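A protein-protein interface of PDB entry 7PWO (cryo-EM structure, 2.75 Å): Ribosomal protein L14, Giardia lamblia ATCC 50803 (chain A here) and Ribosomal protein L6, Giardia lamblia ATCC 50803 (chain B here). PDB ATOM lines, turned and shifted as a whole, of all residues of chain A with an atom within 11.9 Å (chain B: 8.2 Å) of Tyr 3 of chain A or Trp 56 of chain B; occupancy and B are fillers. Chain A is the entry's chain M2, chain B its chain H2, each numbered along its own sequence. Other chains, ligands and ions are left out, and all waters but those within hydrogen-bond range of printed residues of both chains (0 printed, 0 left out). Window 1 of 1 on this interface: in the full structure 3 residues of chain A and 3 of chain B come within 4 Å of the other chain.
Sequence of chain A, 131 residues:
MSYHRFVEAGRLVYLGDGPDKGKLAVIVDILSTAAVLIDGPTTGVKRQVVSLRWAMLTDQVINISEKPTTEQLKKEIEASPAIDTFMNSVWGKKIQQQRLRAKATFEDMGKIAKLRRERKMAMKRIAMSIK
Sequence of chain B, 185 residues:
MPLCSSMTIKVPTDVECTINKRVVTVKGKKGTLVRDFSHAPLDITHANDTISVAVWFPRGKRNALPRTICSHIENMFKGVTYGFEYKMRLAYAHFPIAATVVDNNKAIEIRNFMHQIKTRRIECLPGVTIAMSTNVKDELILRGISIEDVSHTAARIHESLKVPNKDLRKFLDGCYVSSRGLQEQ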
ATOM      1  N   SER A   2      15.118 -33.531   3.922  1.00  0.00           N
ATOM      2  CA  SER A   2      16.298 -33.862   3.129  1.00  0.00           C
ATOM      3  C   SER A   2      15.970 -34.907   2.068  1.00  0.00           C
ATOM      4  O   SER A   2      16.327 -36.072   2.206  1.00  0.00           O
ATOM      5  CB  SER A   2      17.426 -34.363   4.036  1.00  0.00           C
ATOM      6  OG  SER A   2      17.144 -35.660   4.538  1.00  0.00           O
ATOM      7  N   TYR A   3      15.321 -34.467   0.990  1.00  0.00           N
ATOM      8  CA  TYR A   3      14.682 -35.368   0.041  1.00  0.00           C
ATOM      9  C   TYR A   3      15.694 -36.107  -0.831  1.00  0.00           C
ATOM     10  O   TYR A   3      16.881 -35.780  -0.887  1.00  0.00           O
ATOM     11  CB  TYR A   3      13.704 -34.604  -0.845  1.00  0.00           C
ATOM     12  CG  TYR A   3      12.818 -33.638  -0.107  1.00  0.00           C
ATOM     13  CD1 TYR A   3      13.216 -32.334   0.128  1.00  0.00           C
ATOM     14  CD2 TYR A   3      11.578 -34.038   0.359  1.00  0.00           C
ATOM     15  CE1 TYR A   3      12.404 -31.466   0.801  1.00  0.00           C
ATOM     16  CE2 TYR A   3      10.761 -33.172   1.024  1.00  0.00           C
ATOM     17  CZ  TYR A   3      11.177 -31.887   1.243  1.00  0.00           C
ATOM     18  OH  TYR A   3      10.356 -31.022   1.910  1.00  0.00           O
ATOM     19  N   HIS A   4      15.193 -37.135  -1.521  1.00  0.00           N
ATOM     20  CA  HIS A   4      15.994 -37.936  -2.435  1.00  0.00           C
ATOM     21  C   HIS A   4      15.338 -38.192  -3.788  1.00  0.00           C
ATOM     22  O   HIS A   4      16.064 -38.463  -4.751  1.00  0.00           O
ATOM     23  CB  HIS A   4      16.351 -39.283  -1.788  1.00  0.00           C
ATOM     24  CG  HIS A   4      17.459 -39.191  -0.783  1.00  0.00           C
ATOM     25  ND1 HIS A   4      17.244 -39.302   0.573  1.00  0.00           N
ATOM     26  CD2 HIS A   4      18.789 -38.986  -0.936  1.00  0.00           C
ATOM     27  CE1 HIS A   4      18.393 -39.175   1.211  1.00  0.00           C
ATOM     28  NE2 HIS A   4      19.345 -38.980   0.319  1.00  0.00           N
ATOM     29  N   ARG A   5      14.014 -38.111  -3.903  1.00  0.00           N
ATOM     30  CA  ARG A   5      13.317 -38.206  -5.183  1.00  0.00           C
ATOM     31  C   ARG A   5      12.822 -36.825  -5.599  1.00  0.00           C
ATOM     32  O   ARG A   5      12.384 -36.037  -4.759  1.00  0.00           O
ATOM     33  CB  ARG A   5      12.141 -39.176  -5.108  1.00  0.00           C
ATOM     34  CG  ARG A   5      12.513 -40.560  -4.630  1.00  0.00           C
ATOM     35  CD  ARG A   5      11.357 -41.249  -3.958  1.00  0.00           C
ATOM     36  NE  ARG A   5      11.741 -42.569  -3.467  1.00  0.00           N
ATOM     37  CZ  ARG A   5      10.979 -43.652  -3.542  1.00  0.00           C
ATOM     38  NH1 ARG A   5       9.771 -43.581  -4.077  1.00  0.00           N
ATOM     39  NH2 ARG A   5      11.424 -44.805  -3.070  1.00  0.00           N
ATOM     40  N   PHE A   6      12.906 -36.537  -6.897  1.00  0.00           N
ATOM     41  CA  PHE A   6      12.656 -35.208  -7.430  1.00  0.00           C
ATOM     42  C   PHE A   6      11.877 -35.300  -8.734  1.00  0.00           C
ATOM     43  O   PHE A   6      11.980 -36.280  -9.468  1.00  0.00           O
ATOM     44  CB  PHE A   6      13.976 -34.457  -7.663  1.00  0.00           C
ATOM     45  CG  PHE A   6      14.622 -33.971  -6.406  1.00  0.00           C
ATOM     46  CD1 PHE A   6      14.212 -32.792  -5.812  1.00  0.00           C
ATOM     47  CD2 PHE A   6      15.618 -34.704  -5.799  1.00  0.00           C
ATOM     48  CE1 PHE A   6      14.798 -32.345  -4.652  1.00  0.00           C
ATOM     49  CE2 PHE A   6      16.206 -34.259  -4.626  1.00  0.00           C
ATOM     50  CZ  PHE A   6      15.791 -33.080  -4.055  1.00  0.00           C
ATOM     51  N   VAL A   7      11.090 -34.264  -9.006  1.00  0.00           N
ATOM     52  CA  VAL A   7      10.367 -34.126 -10.265  1.00  0.00           C
ATOM     53  C   VAL A   7      11.318 -33.484 -11.269  1.00  0.00           C
ATOM     54  O   VAL A   7      11.829 -32.385 -11.031  1.00  0.00           O
ATOM     55  CB  VAL A   7       9.098 -33.275 -10.085  1.00  0.00           C
ATOM     56  CG1 VAL A   7       8.409 -33.058 -11.416  1.00  0.00           C
ATOM     57  CG2 VAL A   7       8.161 -33.906  -9.102  1.00  0.00           C
ATOM     58  N   GLU A   8      11.555 -34.162 -12.384  1.00  0.00           N
ATOM     59  CA  GLU A   8      12.602 -33.766 -13.315  1.00  0.00           C
ATOM     60  C   GLU A   8      12.556 -34.676 -14.530  1.00  0.00           C
ATOM     61  O   GLU A   8      11.978 -35.765 -14.492  1.00  0.00           O
ATOM     62  CB  GLU A   8      13.990 -33.816 -12.667  1.00  0.00           C
ATOM     63  CG  GLU A   8      14.434 -35.204 -12.267  1.00  0.00           C
ATOM     64  CD  GLU A   8      15.776 -35.202 -11.577  1.00  0.00           C
ATOM     65  OE1 GLU A   8      16.343 -34.105 -11.403  1.00  0.00           O
ATOM     66  OE2 GLU A   8      16.248 -36.279 -11.169  1.00  0.00           O
ATOM     67  N   ARG A  11      12.630 -38.902 -14.917  1.00  0.00           N
ATOM     68  CA  ARG A  11      12.162 -39.625 -13.745  1.00  0.00           C
ATOM     69  C   ARG A  11      11.121 -40.660 -14.142  1.00  0.00           C
ATOM     70  O   ARG A  11      10.181 -40.362 -14.888  1.00  0.00           O
ATOM     71  CB  ARG A  11      11.568 -38.669 -12.714  1.00  0.00           C
ATOM     72  CG  ARG A  11      11.025 -39.365 -11.465  1.00  0.00           C
ATOM     73  CD  ARG A  11      12.092 -40.058 -10.623  1.00  0.00           C
ATOM     74  NE  ARG A  11      13.155 -39.147 -10.216  1.00  0.00           N
ATOM     75  CZ  ARG A  11      13.987 -39.371  -9.203  1.00  0.00           C
ATOM     76  NH1 ARG A  11      13.884 -40.480  -8.493  1.00  0.00           N
ATOM     77  NH2 ARG A  11      14.924 -38.481  -8.899  1.00  0.00           N
ATOM     78  N   ILE A  30       7.703 -30.703 -17.926  1.00  0.00           N
ATOM     79  CA  ILE A  30       7.239 -30.193 -16.634  1.00  0.00           C
ATOM     80  C   ILE A  30       6.445 -28.920 -16.891  1.00  0.00           C
ATOM     81  O   ILE A  30       7.033 -27.882 -17.208  1.00  0.00           O
ATOM     82  CB  ILE A  30       8.413 -29.902 -15.688  1.00  0.00           C
ATOM     83  CG1 ILE A  30       9.267 -31.153 -15.488  1.00  0.00           C
ATOM     84  CG2 ILE A  30       7.912 -29.367 -14.346  1.00  0.00           C
ATOM     85  CD1 ILE A  30       8.521 -32.292 -14.913  1.00  0.00           C
ATOM     86  N   THR A  33       3.729 -26.567 -11.242  1.00  0.00           N
ATOM     87  CA  THR A  33       3.762 -27.387 -10.039  1.00  0.00           C
ATOM     88  C   THR A  33       2.557 -28.328  -9.927  1.00  0.00           C
ATOM     89  O   THR A  33       2.373 -28.885  -8.854  1.00  0.00           O
ATOM     90  CB  THR A  33       3.846 -26.502  -8.795  1.00  0.00           C
ATOM     91  OG1 THR A  33       2.819 -25.501  -8.834  1.00  0.00           O
ATOM     92  CG2 THR A  33       5.212 -25.823  -8.711  1.00  0.00           C
ATOM     93  N   LEU A  57       6.304 -41.133  -7.509  1.00  0.00           N
ATOM     94  CA  LEU A  57       7.707 -41.005  -7.889  1.00  0.00           C
ATOM     95  C   LEU A  57       8.499 -42.256  -7.536  1.00  0.00           C
ATOM     96  O   LEU A  57       8.567 -42.649  -6.371  1.00  0.00           O
ATOM     97  CB  LEU A  57       8.321 -39.793  -7.193  1.00  0.00           C
ATOM     98  CG  LEU A  57       7.933 -38.398  -7.660  1.00  0.00           C
ATOM     99  CD1 LEU A  57       8.727 -37.364  -6.879  1.00  0.00           C
ATOM    100  CD2 LEU A  57       8.113 -38.242  -9.157  1.00  0.00           C
ATOM    101  N   THR A  58       9.103 -42.877  -8.541  1.00  0.00           N
ATOM    102  CA  THR A  58      10.081 -43.934  -8.333  1.00  0.00           C
ATOM    103  C   THR A  58      11.416 -43.290  -7.952  1.00  0.00           C
ATOM    104  O   THR A  58      11.526 -42.067  -7.823  1.00  0.00           O
ATOM    105  CB  THR A  58      10.184 -44.797  -9.592  1.00  0.00           C
ATOM    106  OG1 THR A  58       8.869 -45.058 -10.094  1.00  0.00           O
ATOM    107  CG2 THR A  58      10.823 -46.130  -9.301  1.00  0.00           C
ATOM    108  N   ASP A  59      12.452 -44.102  -7.762  1.00  0.00           N
ATOM    109  CA  ASP A  59      13.776 -43.584  -7.450  1.00  0.00           C
ATOM    110  C   ASP A  59      14.732 -43.578  -8.640  1.00  0.00           C
ATOM    111  O   ASP A  59      15.905 -43.239  -8.467  1.00  0.00           O
ATOM    112  CB  ASP A  59      14.391 -44.367  -6.282  1.00  0.00           C
ATOM    113  CG  ASP A  59      14.470 -45.859  -6.544  1.00  0.00           C
ATOM    114  OD1 ASP A  59      14.627 -46.276  -7.713  1.00  0.00           O
ATOM    115  OD2 ASP A  59      14.360 -46.625  -5.566  1.00  0.00           O
ATOM    116  N   VAL A  61      16.151 -42.350 -12.387  1.00  0.00           N
ATOM    117  CA  VAL A  61      16.207 -41.280 -13.377  1.00  0.00           C
ATOM    118  C   VAL A  61      16.883 -41.829 -14.625  1.00  0.00           C
ATOM    119  O   VAL A  61      18.030 -42.281 -14.563  1.00  0.00           O
ATOM    120  CB  VAL A  61      16.957 -40.047 -12.854  1.00  0.00           C
ATOM    121  CG1 VAL A  61      16.905 -38.932 -13.876  1.00  0.00           C
ATOM    122  CG2 VAL A  61      16.368 -39.583 -11.554  1.00  0.00           C
ATOM    123  N   PRO B   2       9.627 -18.281  -6.659  1.00  0.00           N
ATOM    124  CA  PRO B   2      10.426 -19.440  -7.049  1.00  0.00           C
ATOM    125  C   PRO B   2       9.910 -20.732  -6.438  1.00  0.00           C
ATOM    126  O   PRO B   2       8.849 -20.729  -5.822  1.00  0.00           O
ATOM    127  CB  PRO B   2      11.823 -19.092  -6.526  1.00  0.00           C
ATOM    128  CG  PRO B   2      11.844 -17.618  -6.503  1.00  0.00           C
ATOM    129  CD  PRO B   2      10.463 -17.205  -6.101  1.00  0.00           C
ATOM    130  N   LEU B   3      10.638 -21.828  -6.643  1.00  0.00           N
ATOM    131  CA  LEU B   3      10.314 -23.097  -6.010  1.00  0.00           C
ATOM    132  C   LEU B   3      10.979 -23.260  -4.656  1.00  0.00           C
ATOM    133  O   LEU B   3      10.550 -24.106  -3.866  1.00  0.00           O
ATOM    134  CB  LEU B   3      10.733 -24.269  -6.907  1.00  0.00           C
ATOM    135  CG  LEU B   3      10.208 -24.270  -8.337  1.00  0.00           C
ATOM    136  CD1 LEU B   3      11.064 -25.089  -9.276  1.00  0.00           C
ATOM    137  CD2 LEU B   3       8.769 -24.764  -8.351  1.00  0.00           C
ATOM    138  N   CYS B   4      12.007 -22.471  -4.375  1.00  0.00           N
ATOM    139  CA  CYS B   4      12.758 -22.584  -3.142  1.00  0.00           C
ATOM    140  C   CYS B   4      13.024 -21.185  -2.605  1.00  0.00           C
ATOM    141  O   CYS B   4      12.911 -20.189  -3.319  1.00  0.00           O
ATOM    142  CB  CYS B   4      14.066 -23.347  -3.372  1.00  0.00           C
ATOM    143  SG  CYS B   4      15.068 -23.625  -1.910  1.00  0.00           S
ATOM    144  N   SER B   5      13.336 -21.119  -1.320  1.00  0.00           N
ATOM    145  CA  SER B   5      13.878 -19.906  -0.722  1.00  0.00           C
ATOM    146  C   SER B   5      14.888 -20.331   0.325  1.00  0.00           C
ATOM    147  O   SER B   5      14.555 -21.130   1.201  1.00  0.00           O
ATOM    148  CB  SER B   5      12.778 -19.044  -0.096  1.00  0.00           C
ATOM    149  OG  SER B   5      13.247 -17.743   0.174  1.00  0.00           O
ATOM    150  N   SER B   6      16.106 -19.803   0.247  1.00  0.00           N
ATOM    151  CA  SER B   6      17.195 -20.328   1.057  1.00  0.00           C
ATOM    152  C   SER B   6      18.113 -19.210   1.535  1.00  0.00           C
ATOM    153  O   SER B   6      18.201 -18.141   0.931  1.00  0.00           O
ATOM    154  CB  SER B   6      18.002 -21.375   0.273  1.00  0.00           C
ATOM    155  OG  SER B   6      19.275 -21.567   0.847  1.00  0.00           O
ATOM    156  N   PRO B  41       8.634 -26.353   8.973  1.00  0.00           N
ATOM    157  CA  PRO B  41       9.158 -27.183   7.881  1.00  0.00           C
ATOM    158  C   PRO B  41      10.431 -26.598   7.297  1.00  0.00           C
ATOM    159  O   PRO B  41      10.421 -25.480   6.774  1.00  0.00           O
ATOM    160  CB  PRO B  41       8.020 -27.183   6.851  1.00  0.00           C
ATOM    161  CG  PRO B  41       6.895 -26.398   7.471  1.00  0.00           C
ATOM    162  CD  PRO B  41       7.497 -25.535   8.529  1.00  0.00           C
ATOM    163  N   LEU B  42      11.533 -27.340   7.369  1.00  0.00           N
ATOM    164  CA  LEU B  42      12.842 -26.801   7.038  1.00  0.00           C
ATOM    165  C   LEU B  42      13.641 -27.840   6.272  1.00  0.00           C
ATOM    166  O   LEU B  42      13.461 -29.045   6.462  1.00  0.00           O
ATOM    167  CB  LEU B  42      13.599 -26.407   8.311  1.00  0.00           C
ATOM    168  CG  LEU B  42      13.070 -25.263   9.185  1.00  0.00           C
ATOM    169  CD1 LEU B  42      13.897 -25.163  10.444  1.00  0.00           C
ATOM    170  CD2 LEU B  42      13.068 -23.930   8.458  1.00  0.00           C
ATOM    171  N   ASP B  43      14.550 -27.372   5.422  1.00  0.00           N
ATOM    172  CA  ASP B  43      15.557 -28.234   4.812  1.00  0.00           C
ATOM    173  C   ASP B  43      16.908 -27.623   5.176  1.00  0.00           C
ATOM    174  O   ASP B  43      17.371 -26.690   4.520  1.00  0.00           O
ATOM    175  CB  ASP B  43      15.346 -28.344   3.310  1.00  0.00           C
ATOM    176  CG  ASP B  43      15.982 -29.591   2.716  1.00  0.00           C
ATOM    177  OD1 ASP B  43      16.609 -30.364   3.465  1.00  0.00           O
ATOM    178  OD2 ASP B  43      15.853 -29.794   1.496  1.00  0.00           O
ATOM    179  N   ILE B  44      17.515 -28.120   6.251  1.00  0.00           N
ATOM    180  CA  ILE B  44      18.804 -27.637   6.731  1.00  0.00           C
ATOM    181  C   ILE B  44      19.872 -28.612   6.248  1.00  0.00           C
ATOM    182  O   ILE B  44      19.925 -29.763   6.689  1.00  0.00           O
ATOM    183  CB  ILE B  44      18.824 -27.501   8.258  1.00  0.00           C
ATOM    184  CG1 ILE B  44      17.606 -26.716   8.735  1.00  0.00           C
ATOM    185  CG2 ILE B  44      20.082 -26.799   8.717  1.00  0.00           C
ATOM    186  CD1 ILE B  44      17.142 -27.102  10.102  1.00  0.00           C
ATOM    187  N   THR B  45      20.726 -28.146   5.348  1.00  0.00           N
ATOM    188  CA  THR B  45      21.757 -28.958   4.721  1.00  0.00           C
ATOM    189  C   THR B  45      23.112 -28.571   5.297  1.00  0.00           C
ATOM    190  O   THR B  45      23.441 -27.379   5.385  1.00  0.00           O
ATOM    191  CB  THR B  45      21.760 -28.773   3.202  1.00  0.00           C
ATOM    192  OG1 THR B  45      20.485 -29.154   2.676  1.00  0.00           O
ATOM    193  CG2 THR B  45      22.832 -29.647   2.561  1.00  0.00           C
ATOM    194  N   VAL B  53      19.738 -23.210   4.976  1.00  0.00           N
ATOM    195  CA  VAL B  53      18.351 -23.410   5.394  1.00  0.00           C
ATOM    196  C   VAL B  53      17.454 -23.043   4.224  1.00  0.00           C
ATOM    197  O   VAL B  53      17.537 -21.921   3.706  1.00  0.00           O
ATOM    198  CB  VAL B  53      17.990 -22.573   6.633  1.00  0.00           C
ATOM    199  CG1 VAL B  53      16.684 -23.049   7.230  1.00  0.00           C
ATOM    200  CG2 VAL B  53      19.086 -22.650   7.663  1.00  0.00           C
ATOM    201  N   ALA B  54      16.594 -23.979   3.813  1.00  0.00           N
ATOM    202  CA  ALA B  54      15.777 -23.827   2.620  1.00  0.00           C
ATOM    203  C   ALA B  54      14.329 -24.210   2.894  1.00  0.00           C
ATOM    204  O   ALA B  54      14.032 -25.033   3.763  1.00  0.00           O
ATOM    205  CB  ALA B  54      16.312 -24.675   1.469  1.00  0.00           C
ATOM    206  N   VAL B  55      13.428 -23.592   2.136  1.00  0.00           N
ATOM    207  CA  VAL B  55      11.998 -23.850   2.219  1.00  0.00           C
ATOM    208  C   VAL B  55      11.479 -24.033   0.802  1.00  0.00           C
ATOM    209  O   VAL B  55      11.624 -23.136  -0.034  1.00  0.00           O
ATOM    210  CB  VAL B  55      11.240 -22.717   2.932  1.00  0.00           C
ATOM    211  CG1 VAL B  55       9.760 -22.986   2.901  1.00  0.00           C
ATOM    212  CG2 VAL B  55      11.712 -22.574   4.361  1.00  0.00           C
ATOM    213  N   TRP B  56      10.882 -25.188   0.533  1.00  0.00           N
ATOM    214  CA  TRP B  56      10.303 -25.489  -0.768  1.00  0.00           C
ATOM    215  C   TRP B  56       8.856 -25.031  -0.828  1.00  0.00           C
ATOM    216  O   TRP B  56       8.097 -25.228   0.120  1.00  0.00           O
ATOM    217  CB  TRP B  56      10.369 -26.983  -1.053  1.00  0.00           C
ATOM    218  CG  TRP B  56      11.735 -27.520  -1.254  1.00  0.00           C
ATOM    219  CD1 TRP B  56      12.458 -28.257  -0.372  1.00  0.00           C
ATOM    220  CD2 TRP B  56      12.533 -27.417  -2.439  1.00  0.00           C
ATOM    221  NE1 TRP B  56      13.666 -28.602  -0.920  1.00  0.00           N
ATOM    222  CE2 TRP B  56      13.736 -28.099  -2.190  1.00  0.00           C
ATOM    223  CE3 TRP B  56      12.353 -26.799  -3.677  1.00  0.00           C
ATOM    224  CZ2 TRP B  56      14.748 -28.185  -3.131  1.00  0.00           C
ATOM    225  CZ3 TRP B  56      13.351 -26.885  -4.602  1.00  0.00           C
ATOM    226  CH2 TRP B  56      14.538 -27.575  -4.330  1.00  0.00           C
ATOM    227  N   PHE B  57       8.483 -24.425  -1.951  1.00  0.00           N
ATOM    228  CA  PHE B  57       7.129 -23.971  -2.251  1.00  0.00           C
ATOM    229  C   PHE B  57       6.631 -22.994  -1.198  1.00  0.00           C
ATOM    230  O   PHE B  57       5.742 -23.343  -0.413  1.00  0.00           O
ATOM    231  CB  PHE B  57       6.158 -25.152  -2.319  1.00  0.00           C
ATOM    232  CG  PHE B  57       6.608 -26.262  -3.210  1.00  0.00           C
ATOM    233  CD1 PHE B  57       6.934 -26.023  -4.526  1.00  0.00           C
ATOM    234  CD2 PHE B  57       6.738 -27.546  -2.714  1.00  0.00           C
ATOM    235  CE1 PHE B  57       7.353 -27.050  -5.337  1.00  0.00           C
ATOM    236  CE2 PHE B  57       7.164 -28.568  -3.516  1.00  0.00           C
ATOM    237  CZ  PHE B  57       7.471 -28.321  -4.832  1.00  0.00           C
ATOM    238  N   PRO B  58       7.176 -21.785  -1.124  1.00  0.00           N
ATOM    239  CA  PRO B  58       6.618 -20.788  -0.216  1.00  0.00           C
ATOM    240  C   PRO B  58       5.351 -20.184  -0.797  1.00  0.00           C
ATOM    241  O   PRO B  58       5.129 -20.172  -2.007  1.00  0.00           O
ATOM    242  CB  PRO B  58       7.734 -19.741  -0.107  1.00  0.00           C
ATOM    243  CG  PRO B  58       8.894 -20.299  -0.870  1.00  0.00           C
ATOM    244  CD  PRO B  58       8.334 -21.246  -1.849  1.00  0.00           C
ATOM    245  N   ARG B  59       4.497 -19.696   0.098  1.00  0.00           N
ATOM    246  CA  ARG B  59       3.289 -19.012  -0.334  1.00  0.00           C
ATOM    247  C   ARG B  59       2.946 -17.793   0.512  1.00  0.00           C
ATOM    248  O   ARG B  59       1.976 -17.097   0.203  1.00  0.00           O
ATOM    249  CB  ARG B  59       2.113 -19.996  -0.340  1.00  0.00           C
ATOM    250  CG  ARG B  59       0.952 -19.577  -1.191  1.00  0.00           C
ATOM    251  CD  ARG B  59       0.050 -20.756  -1.527  1.00  0.00           C
ATOM    252  NE  ARG B  59      -1.246 -20.289  -2.004  1.00  0.00           N
ATOM    253  CZ  ARG B  59      -1.451 -19.704  -3.174  1.00  0.00           C
ATOM    254  NH1 ARG B  59      -0.447 -19.535  -4.026  1.00  0.00           N
ATOM    255  NH2 ARG B  59      -2.671 -19.305  -3.501  1.00  0.00           N
ATOM    256  N   ARG B  62       5.816 -18.306   5.078  1.00  0.00           N
ATOM    257  CA  ARG B  62       6.841 -19.342   4.989  1.00  0.00           C
ATOM    258  C   ARG B  62       8.122 -18.822   4.363  1.00  0.00           C
ATOM    259  O   ARG B  62       9.189 -19.394   4.592  1.00  0.00           O
ATOM    260  CB  ARG B  62       6.342 -20.532   4.181  1.00  0.00           C
ATOM    261  CG  ARG B  62       5.065 -21.123   4.672  1.00  0.00           C
ATOM    262  CD  ARG B  62       5.088 -22.625   4.523  1.00  0.00           C
ATOM    263  NE  ARG B  62       4.812 -23.044   3.159  1.00  0.00           N
ATOM    264  CZ  ARG B  62       4.948 -24.292   2.724  1.00  0.00           C
ATOM    265  NH1 ARG B  62       5.347 -25.242   3.550  1.00  0.00           N
ATOM    266  NH2 ARG B  62       4.677 -24.592   1.463  1.00  0.00           N
ATOM    267  N   PRO B  66      13.734 -18.756   6.704  1.00  0.00           N
ATOM    268  CA  PRO B  66      15.159 -19.128   6.643  1.00  0.00           C
ATOM    269  C   PRO B  66      16.090 -18.134   7.319  1.00  0.00           C
ATOM    270  O   PRO B  66      17.038 -18.553   7.997  1.00  0.00           O
ATOM    271  CB  PRO B  66      15.424 -19.244   5.135  1.00  0.00           C
ATOM    272  CG  PRO B  66      14.089 -19.400   4.517  1.00  0.00           C
ATOM    273  CD  PRO B  66      13.184 -18.573   5.348  1.00  0.00           C
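Of the 14 printed residues of chain A, 3 touch a printed residue of chain B. Printed residues of chain A that touch a printed residue of chain B: Ser 2, Tyr 3 and Thr 33. Along chain A the printed residues that touch a printed residue of chain B span positions 2 to 33. Among the printed residues, no Asp or Glu carboxylate lies within 4 Å of a Lys or Arg side-chain nitrogen of the other chain.
Among the printed residues, pairs that only touch across the chains: Tyr 3 of chain A with Trp 56 of chain B (3.4 Å), Ser 2 of chain A with Asp 43 of chain B (3.5 Å), Thr 33 of chain A with Leu 3 of chain B (3.7 Å) and Tyr 3 of chain A with Asp 43 of chain B (3.9 Å).
The backbone NH (N) of Phe 57 of chain B is in hydrogen-bond range of the backbone carbonyl oxygen (O) of Leu 3 of chain B, at 2.8 Å. N of Ala 54 of chain B is in hydrogen-bond range of O of Asp 43 of chain B (2.9 Å). The indole nitrogen (NE1) of Trp 56 of chain B lies within hydrogen-bond range of the side-chain carboxylate (OD2) of Asp 43 of chain B (3.5 Å).
Tyr 3 of chain A touches two residues of chain B. Trp 56 of chain B touches just one residue of chain A: Tyr 3 (3.4 Å). Leu 3 of chain B touches one residue of chain A. No residue of chain A comes within 4 Å of Cys 4 of chain B. No residue of chain A comes within 4 Å of Ser 5 of chain B. Asp 43 of chain B touches two residues of chain A. No residue of chain A comes within 4 Å of Ala 54 of chain B. Val 55 of chain B touches none of the printed residues of chain A. No residue of chain A comes within 4 Å of Phe 57 of chain B. No residue of chain A comes within 4 Å of Pro 58 of chain B. Of the printed residues of chain B, Ser 2 of chain A touches Asp 43. Of the printed residues of chain B, Thr 33 of chain A touches Leu 3 (3.7 Å). Glu 8 of chain A touches none of the printed residues of chain B. The nearest residue of chain B that does not touch Tyr 3 of chain A is Leu 42 of chain B (5.9 Å). The nearest residue of chain A that does not touch Trp 56 of chain B is Phe 6 of chain A (4.4 Å). The nearest printed residue of chain B that does not touch Thr 33 of chain A is Phe 57 of chain B (4.2 Å).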
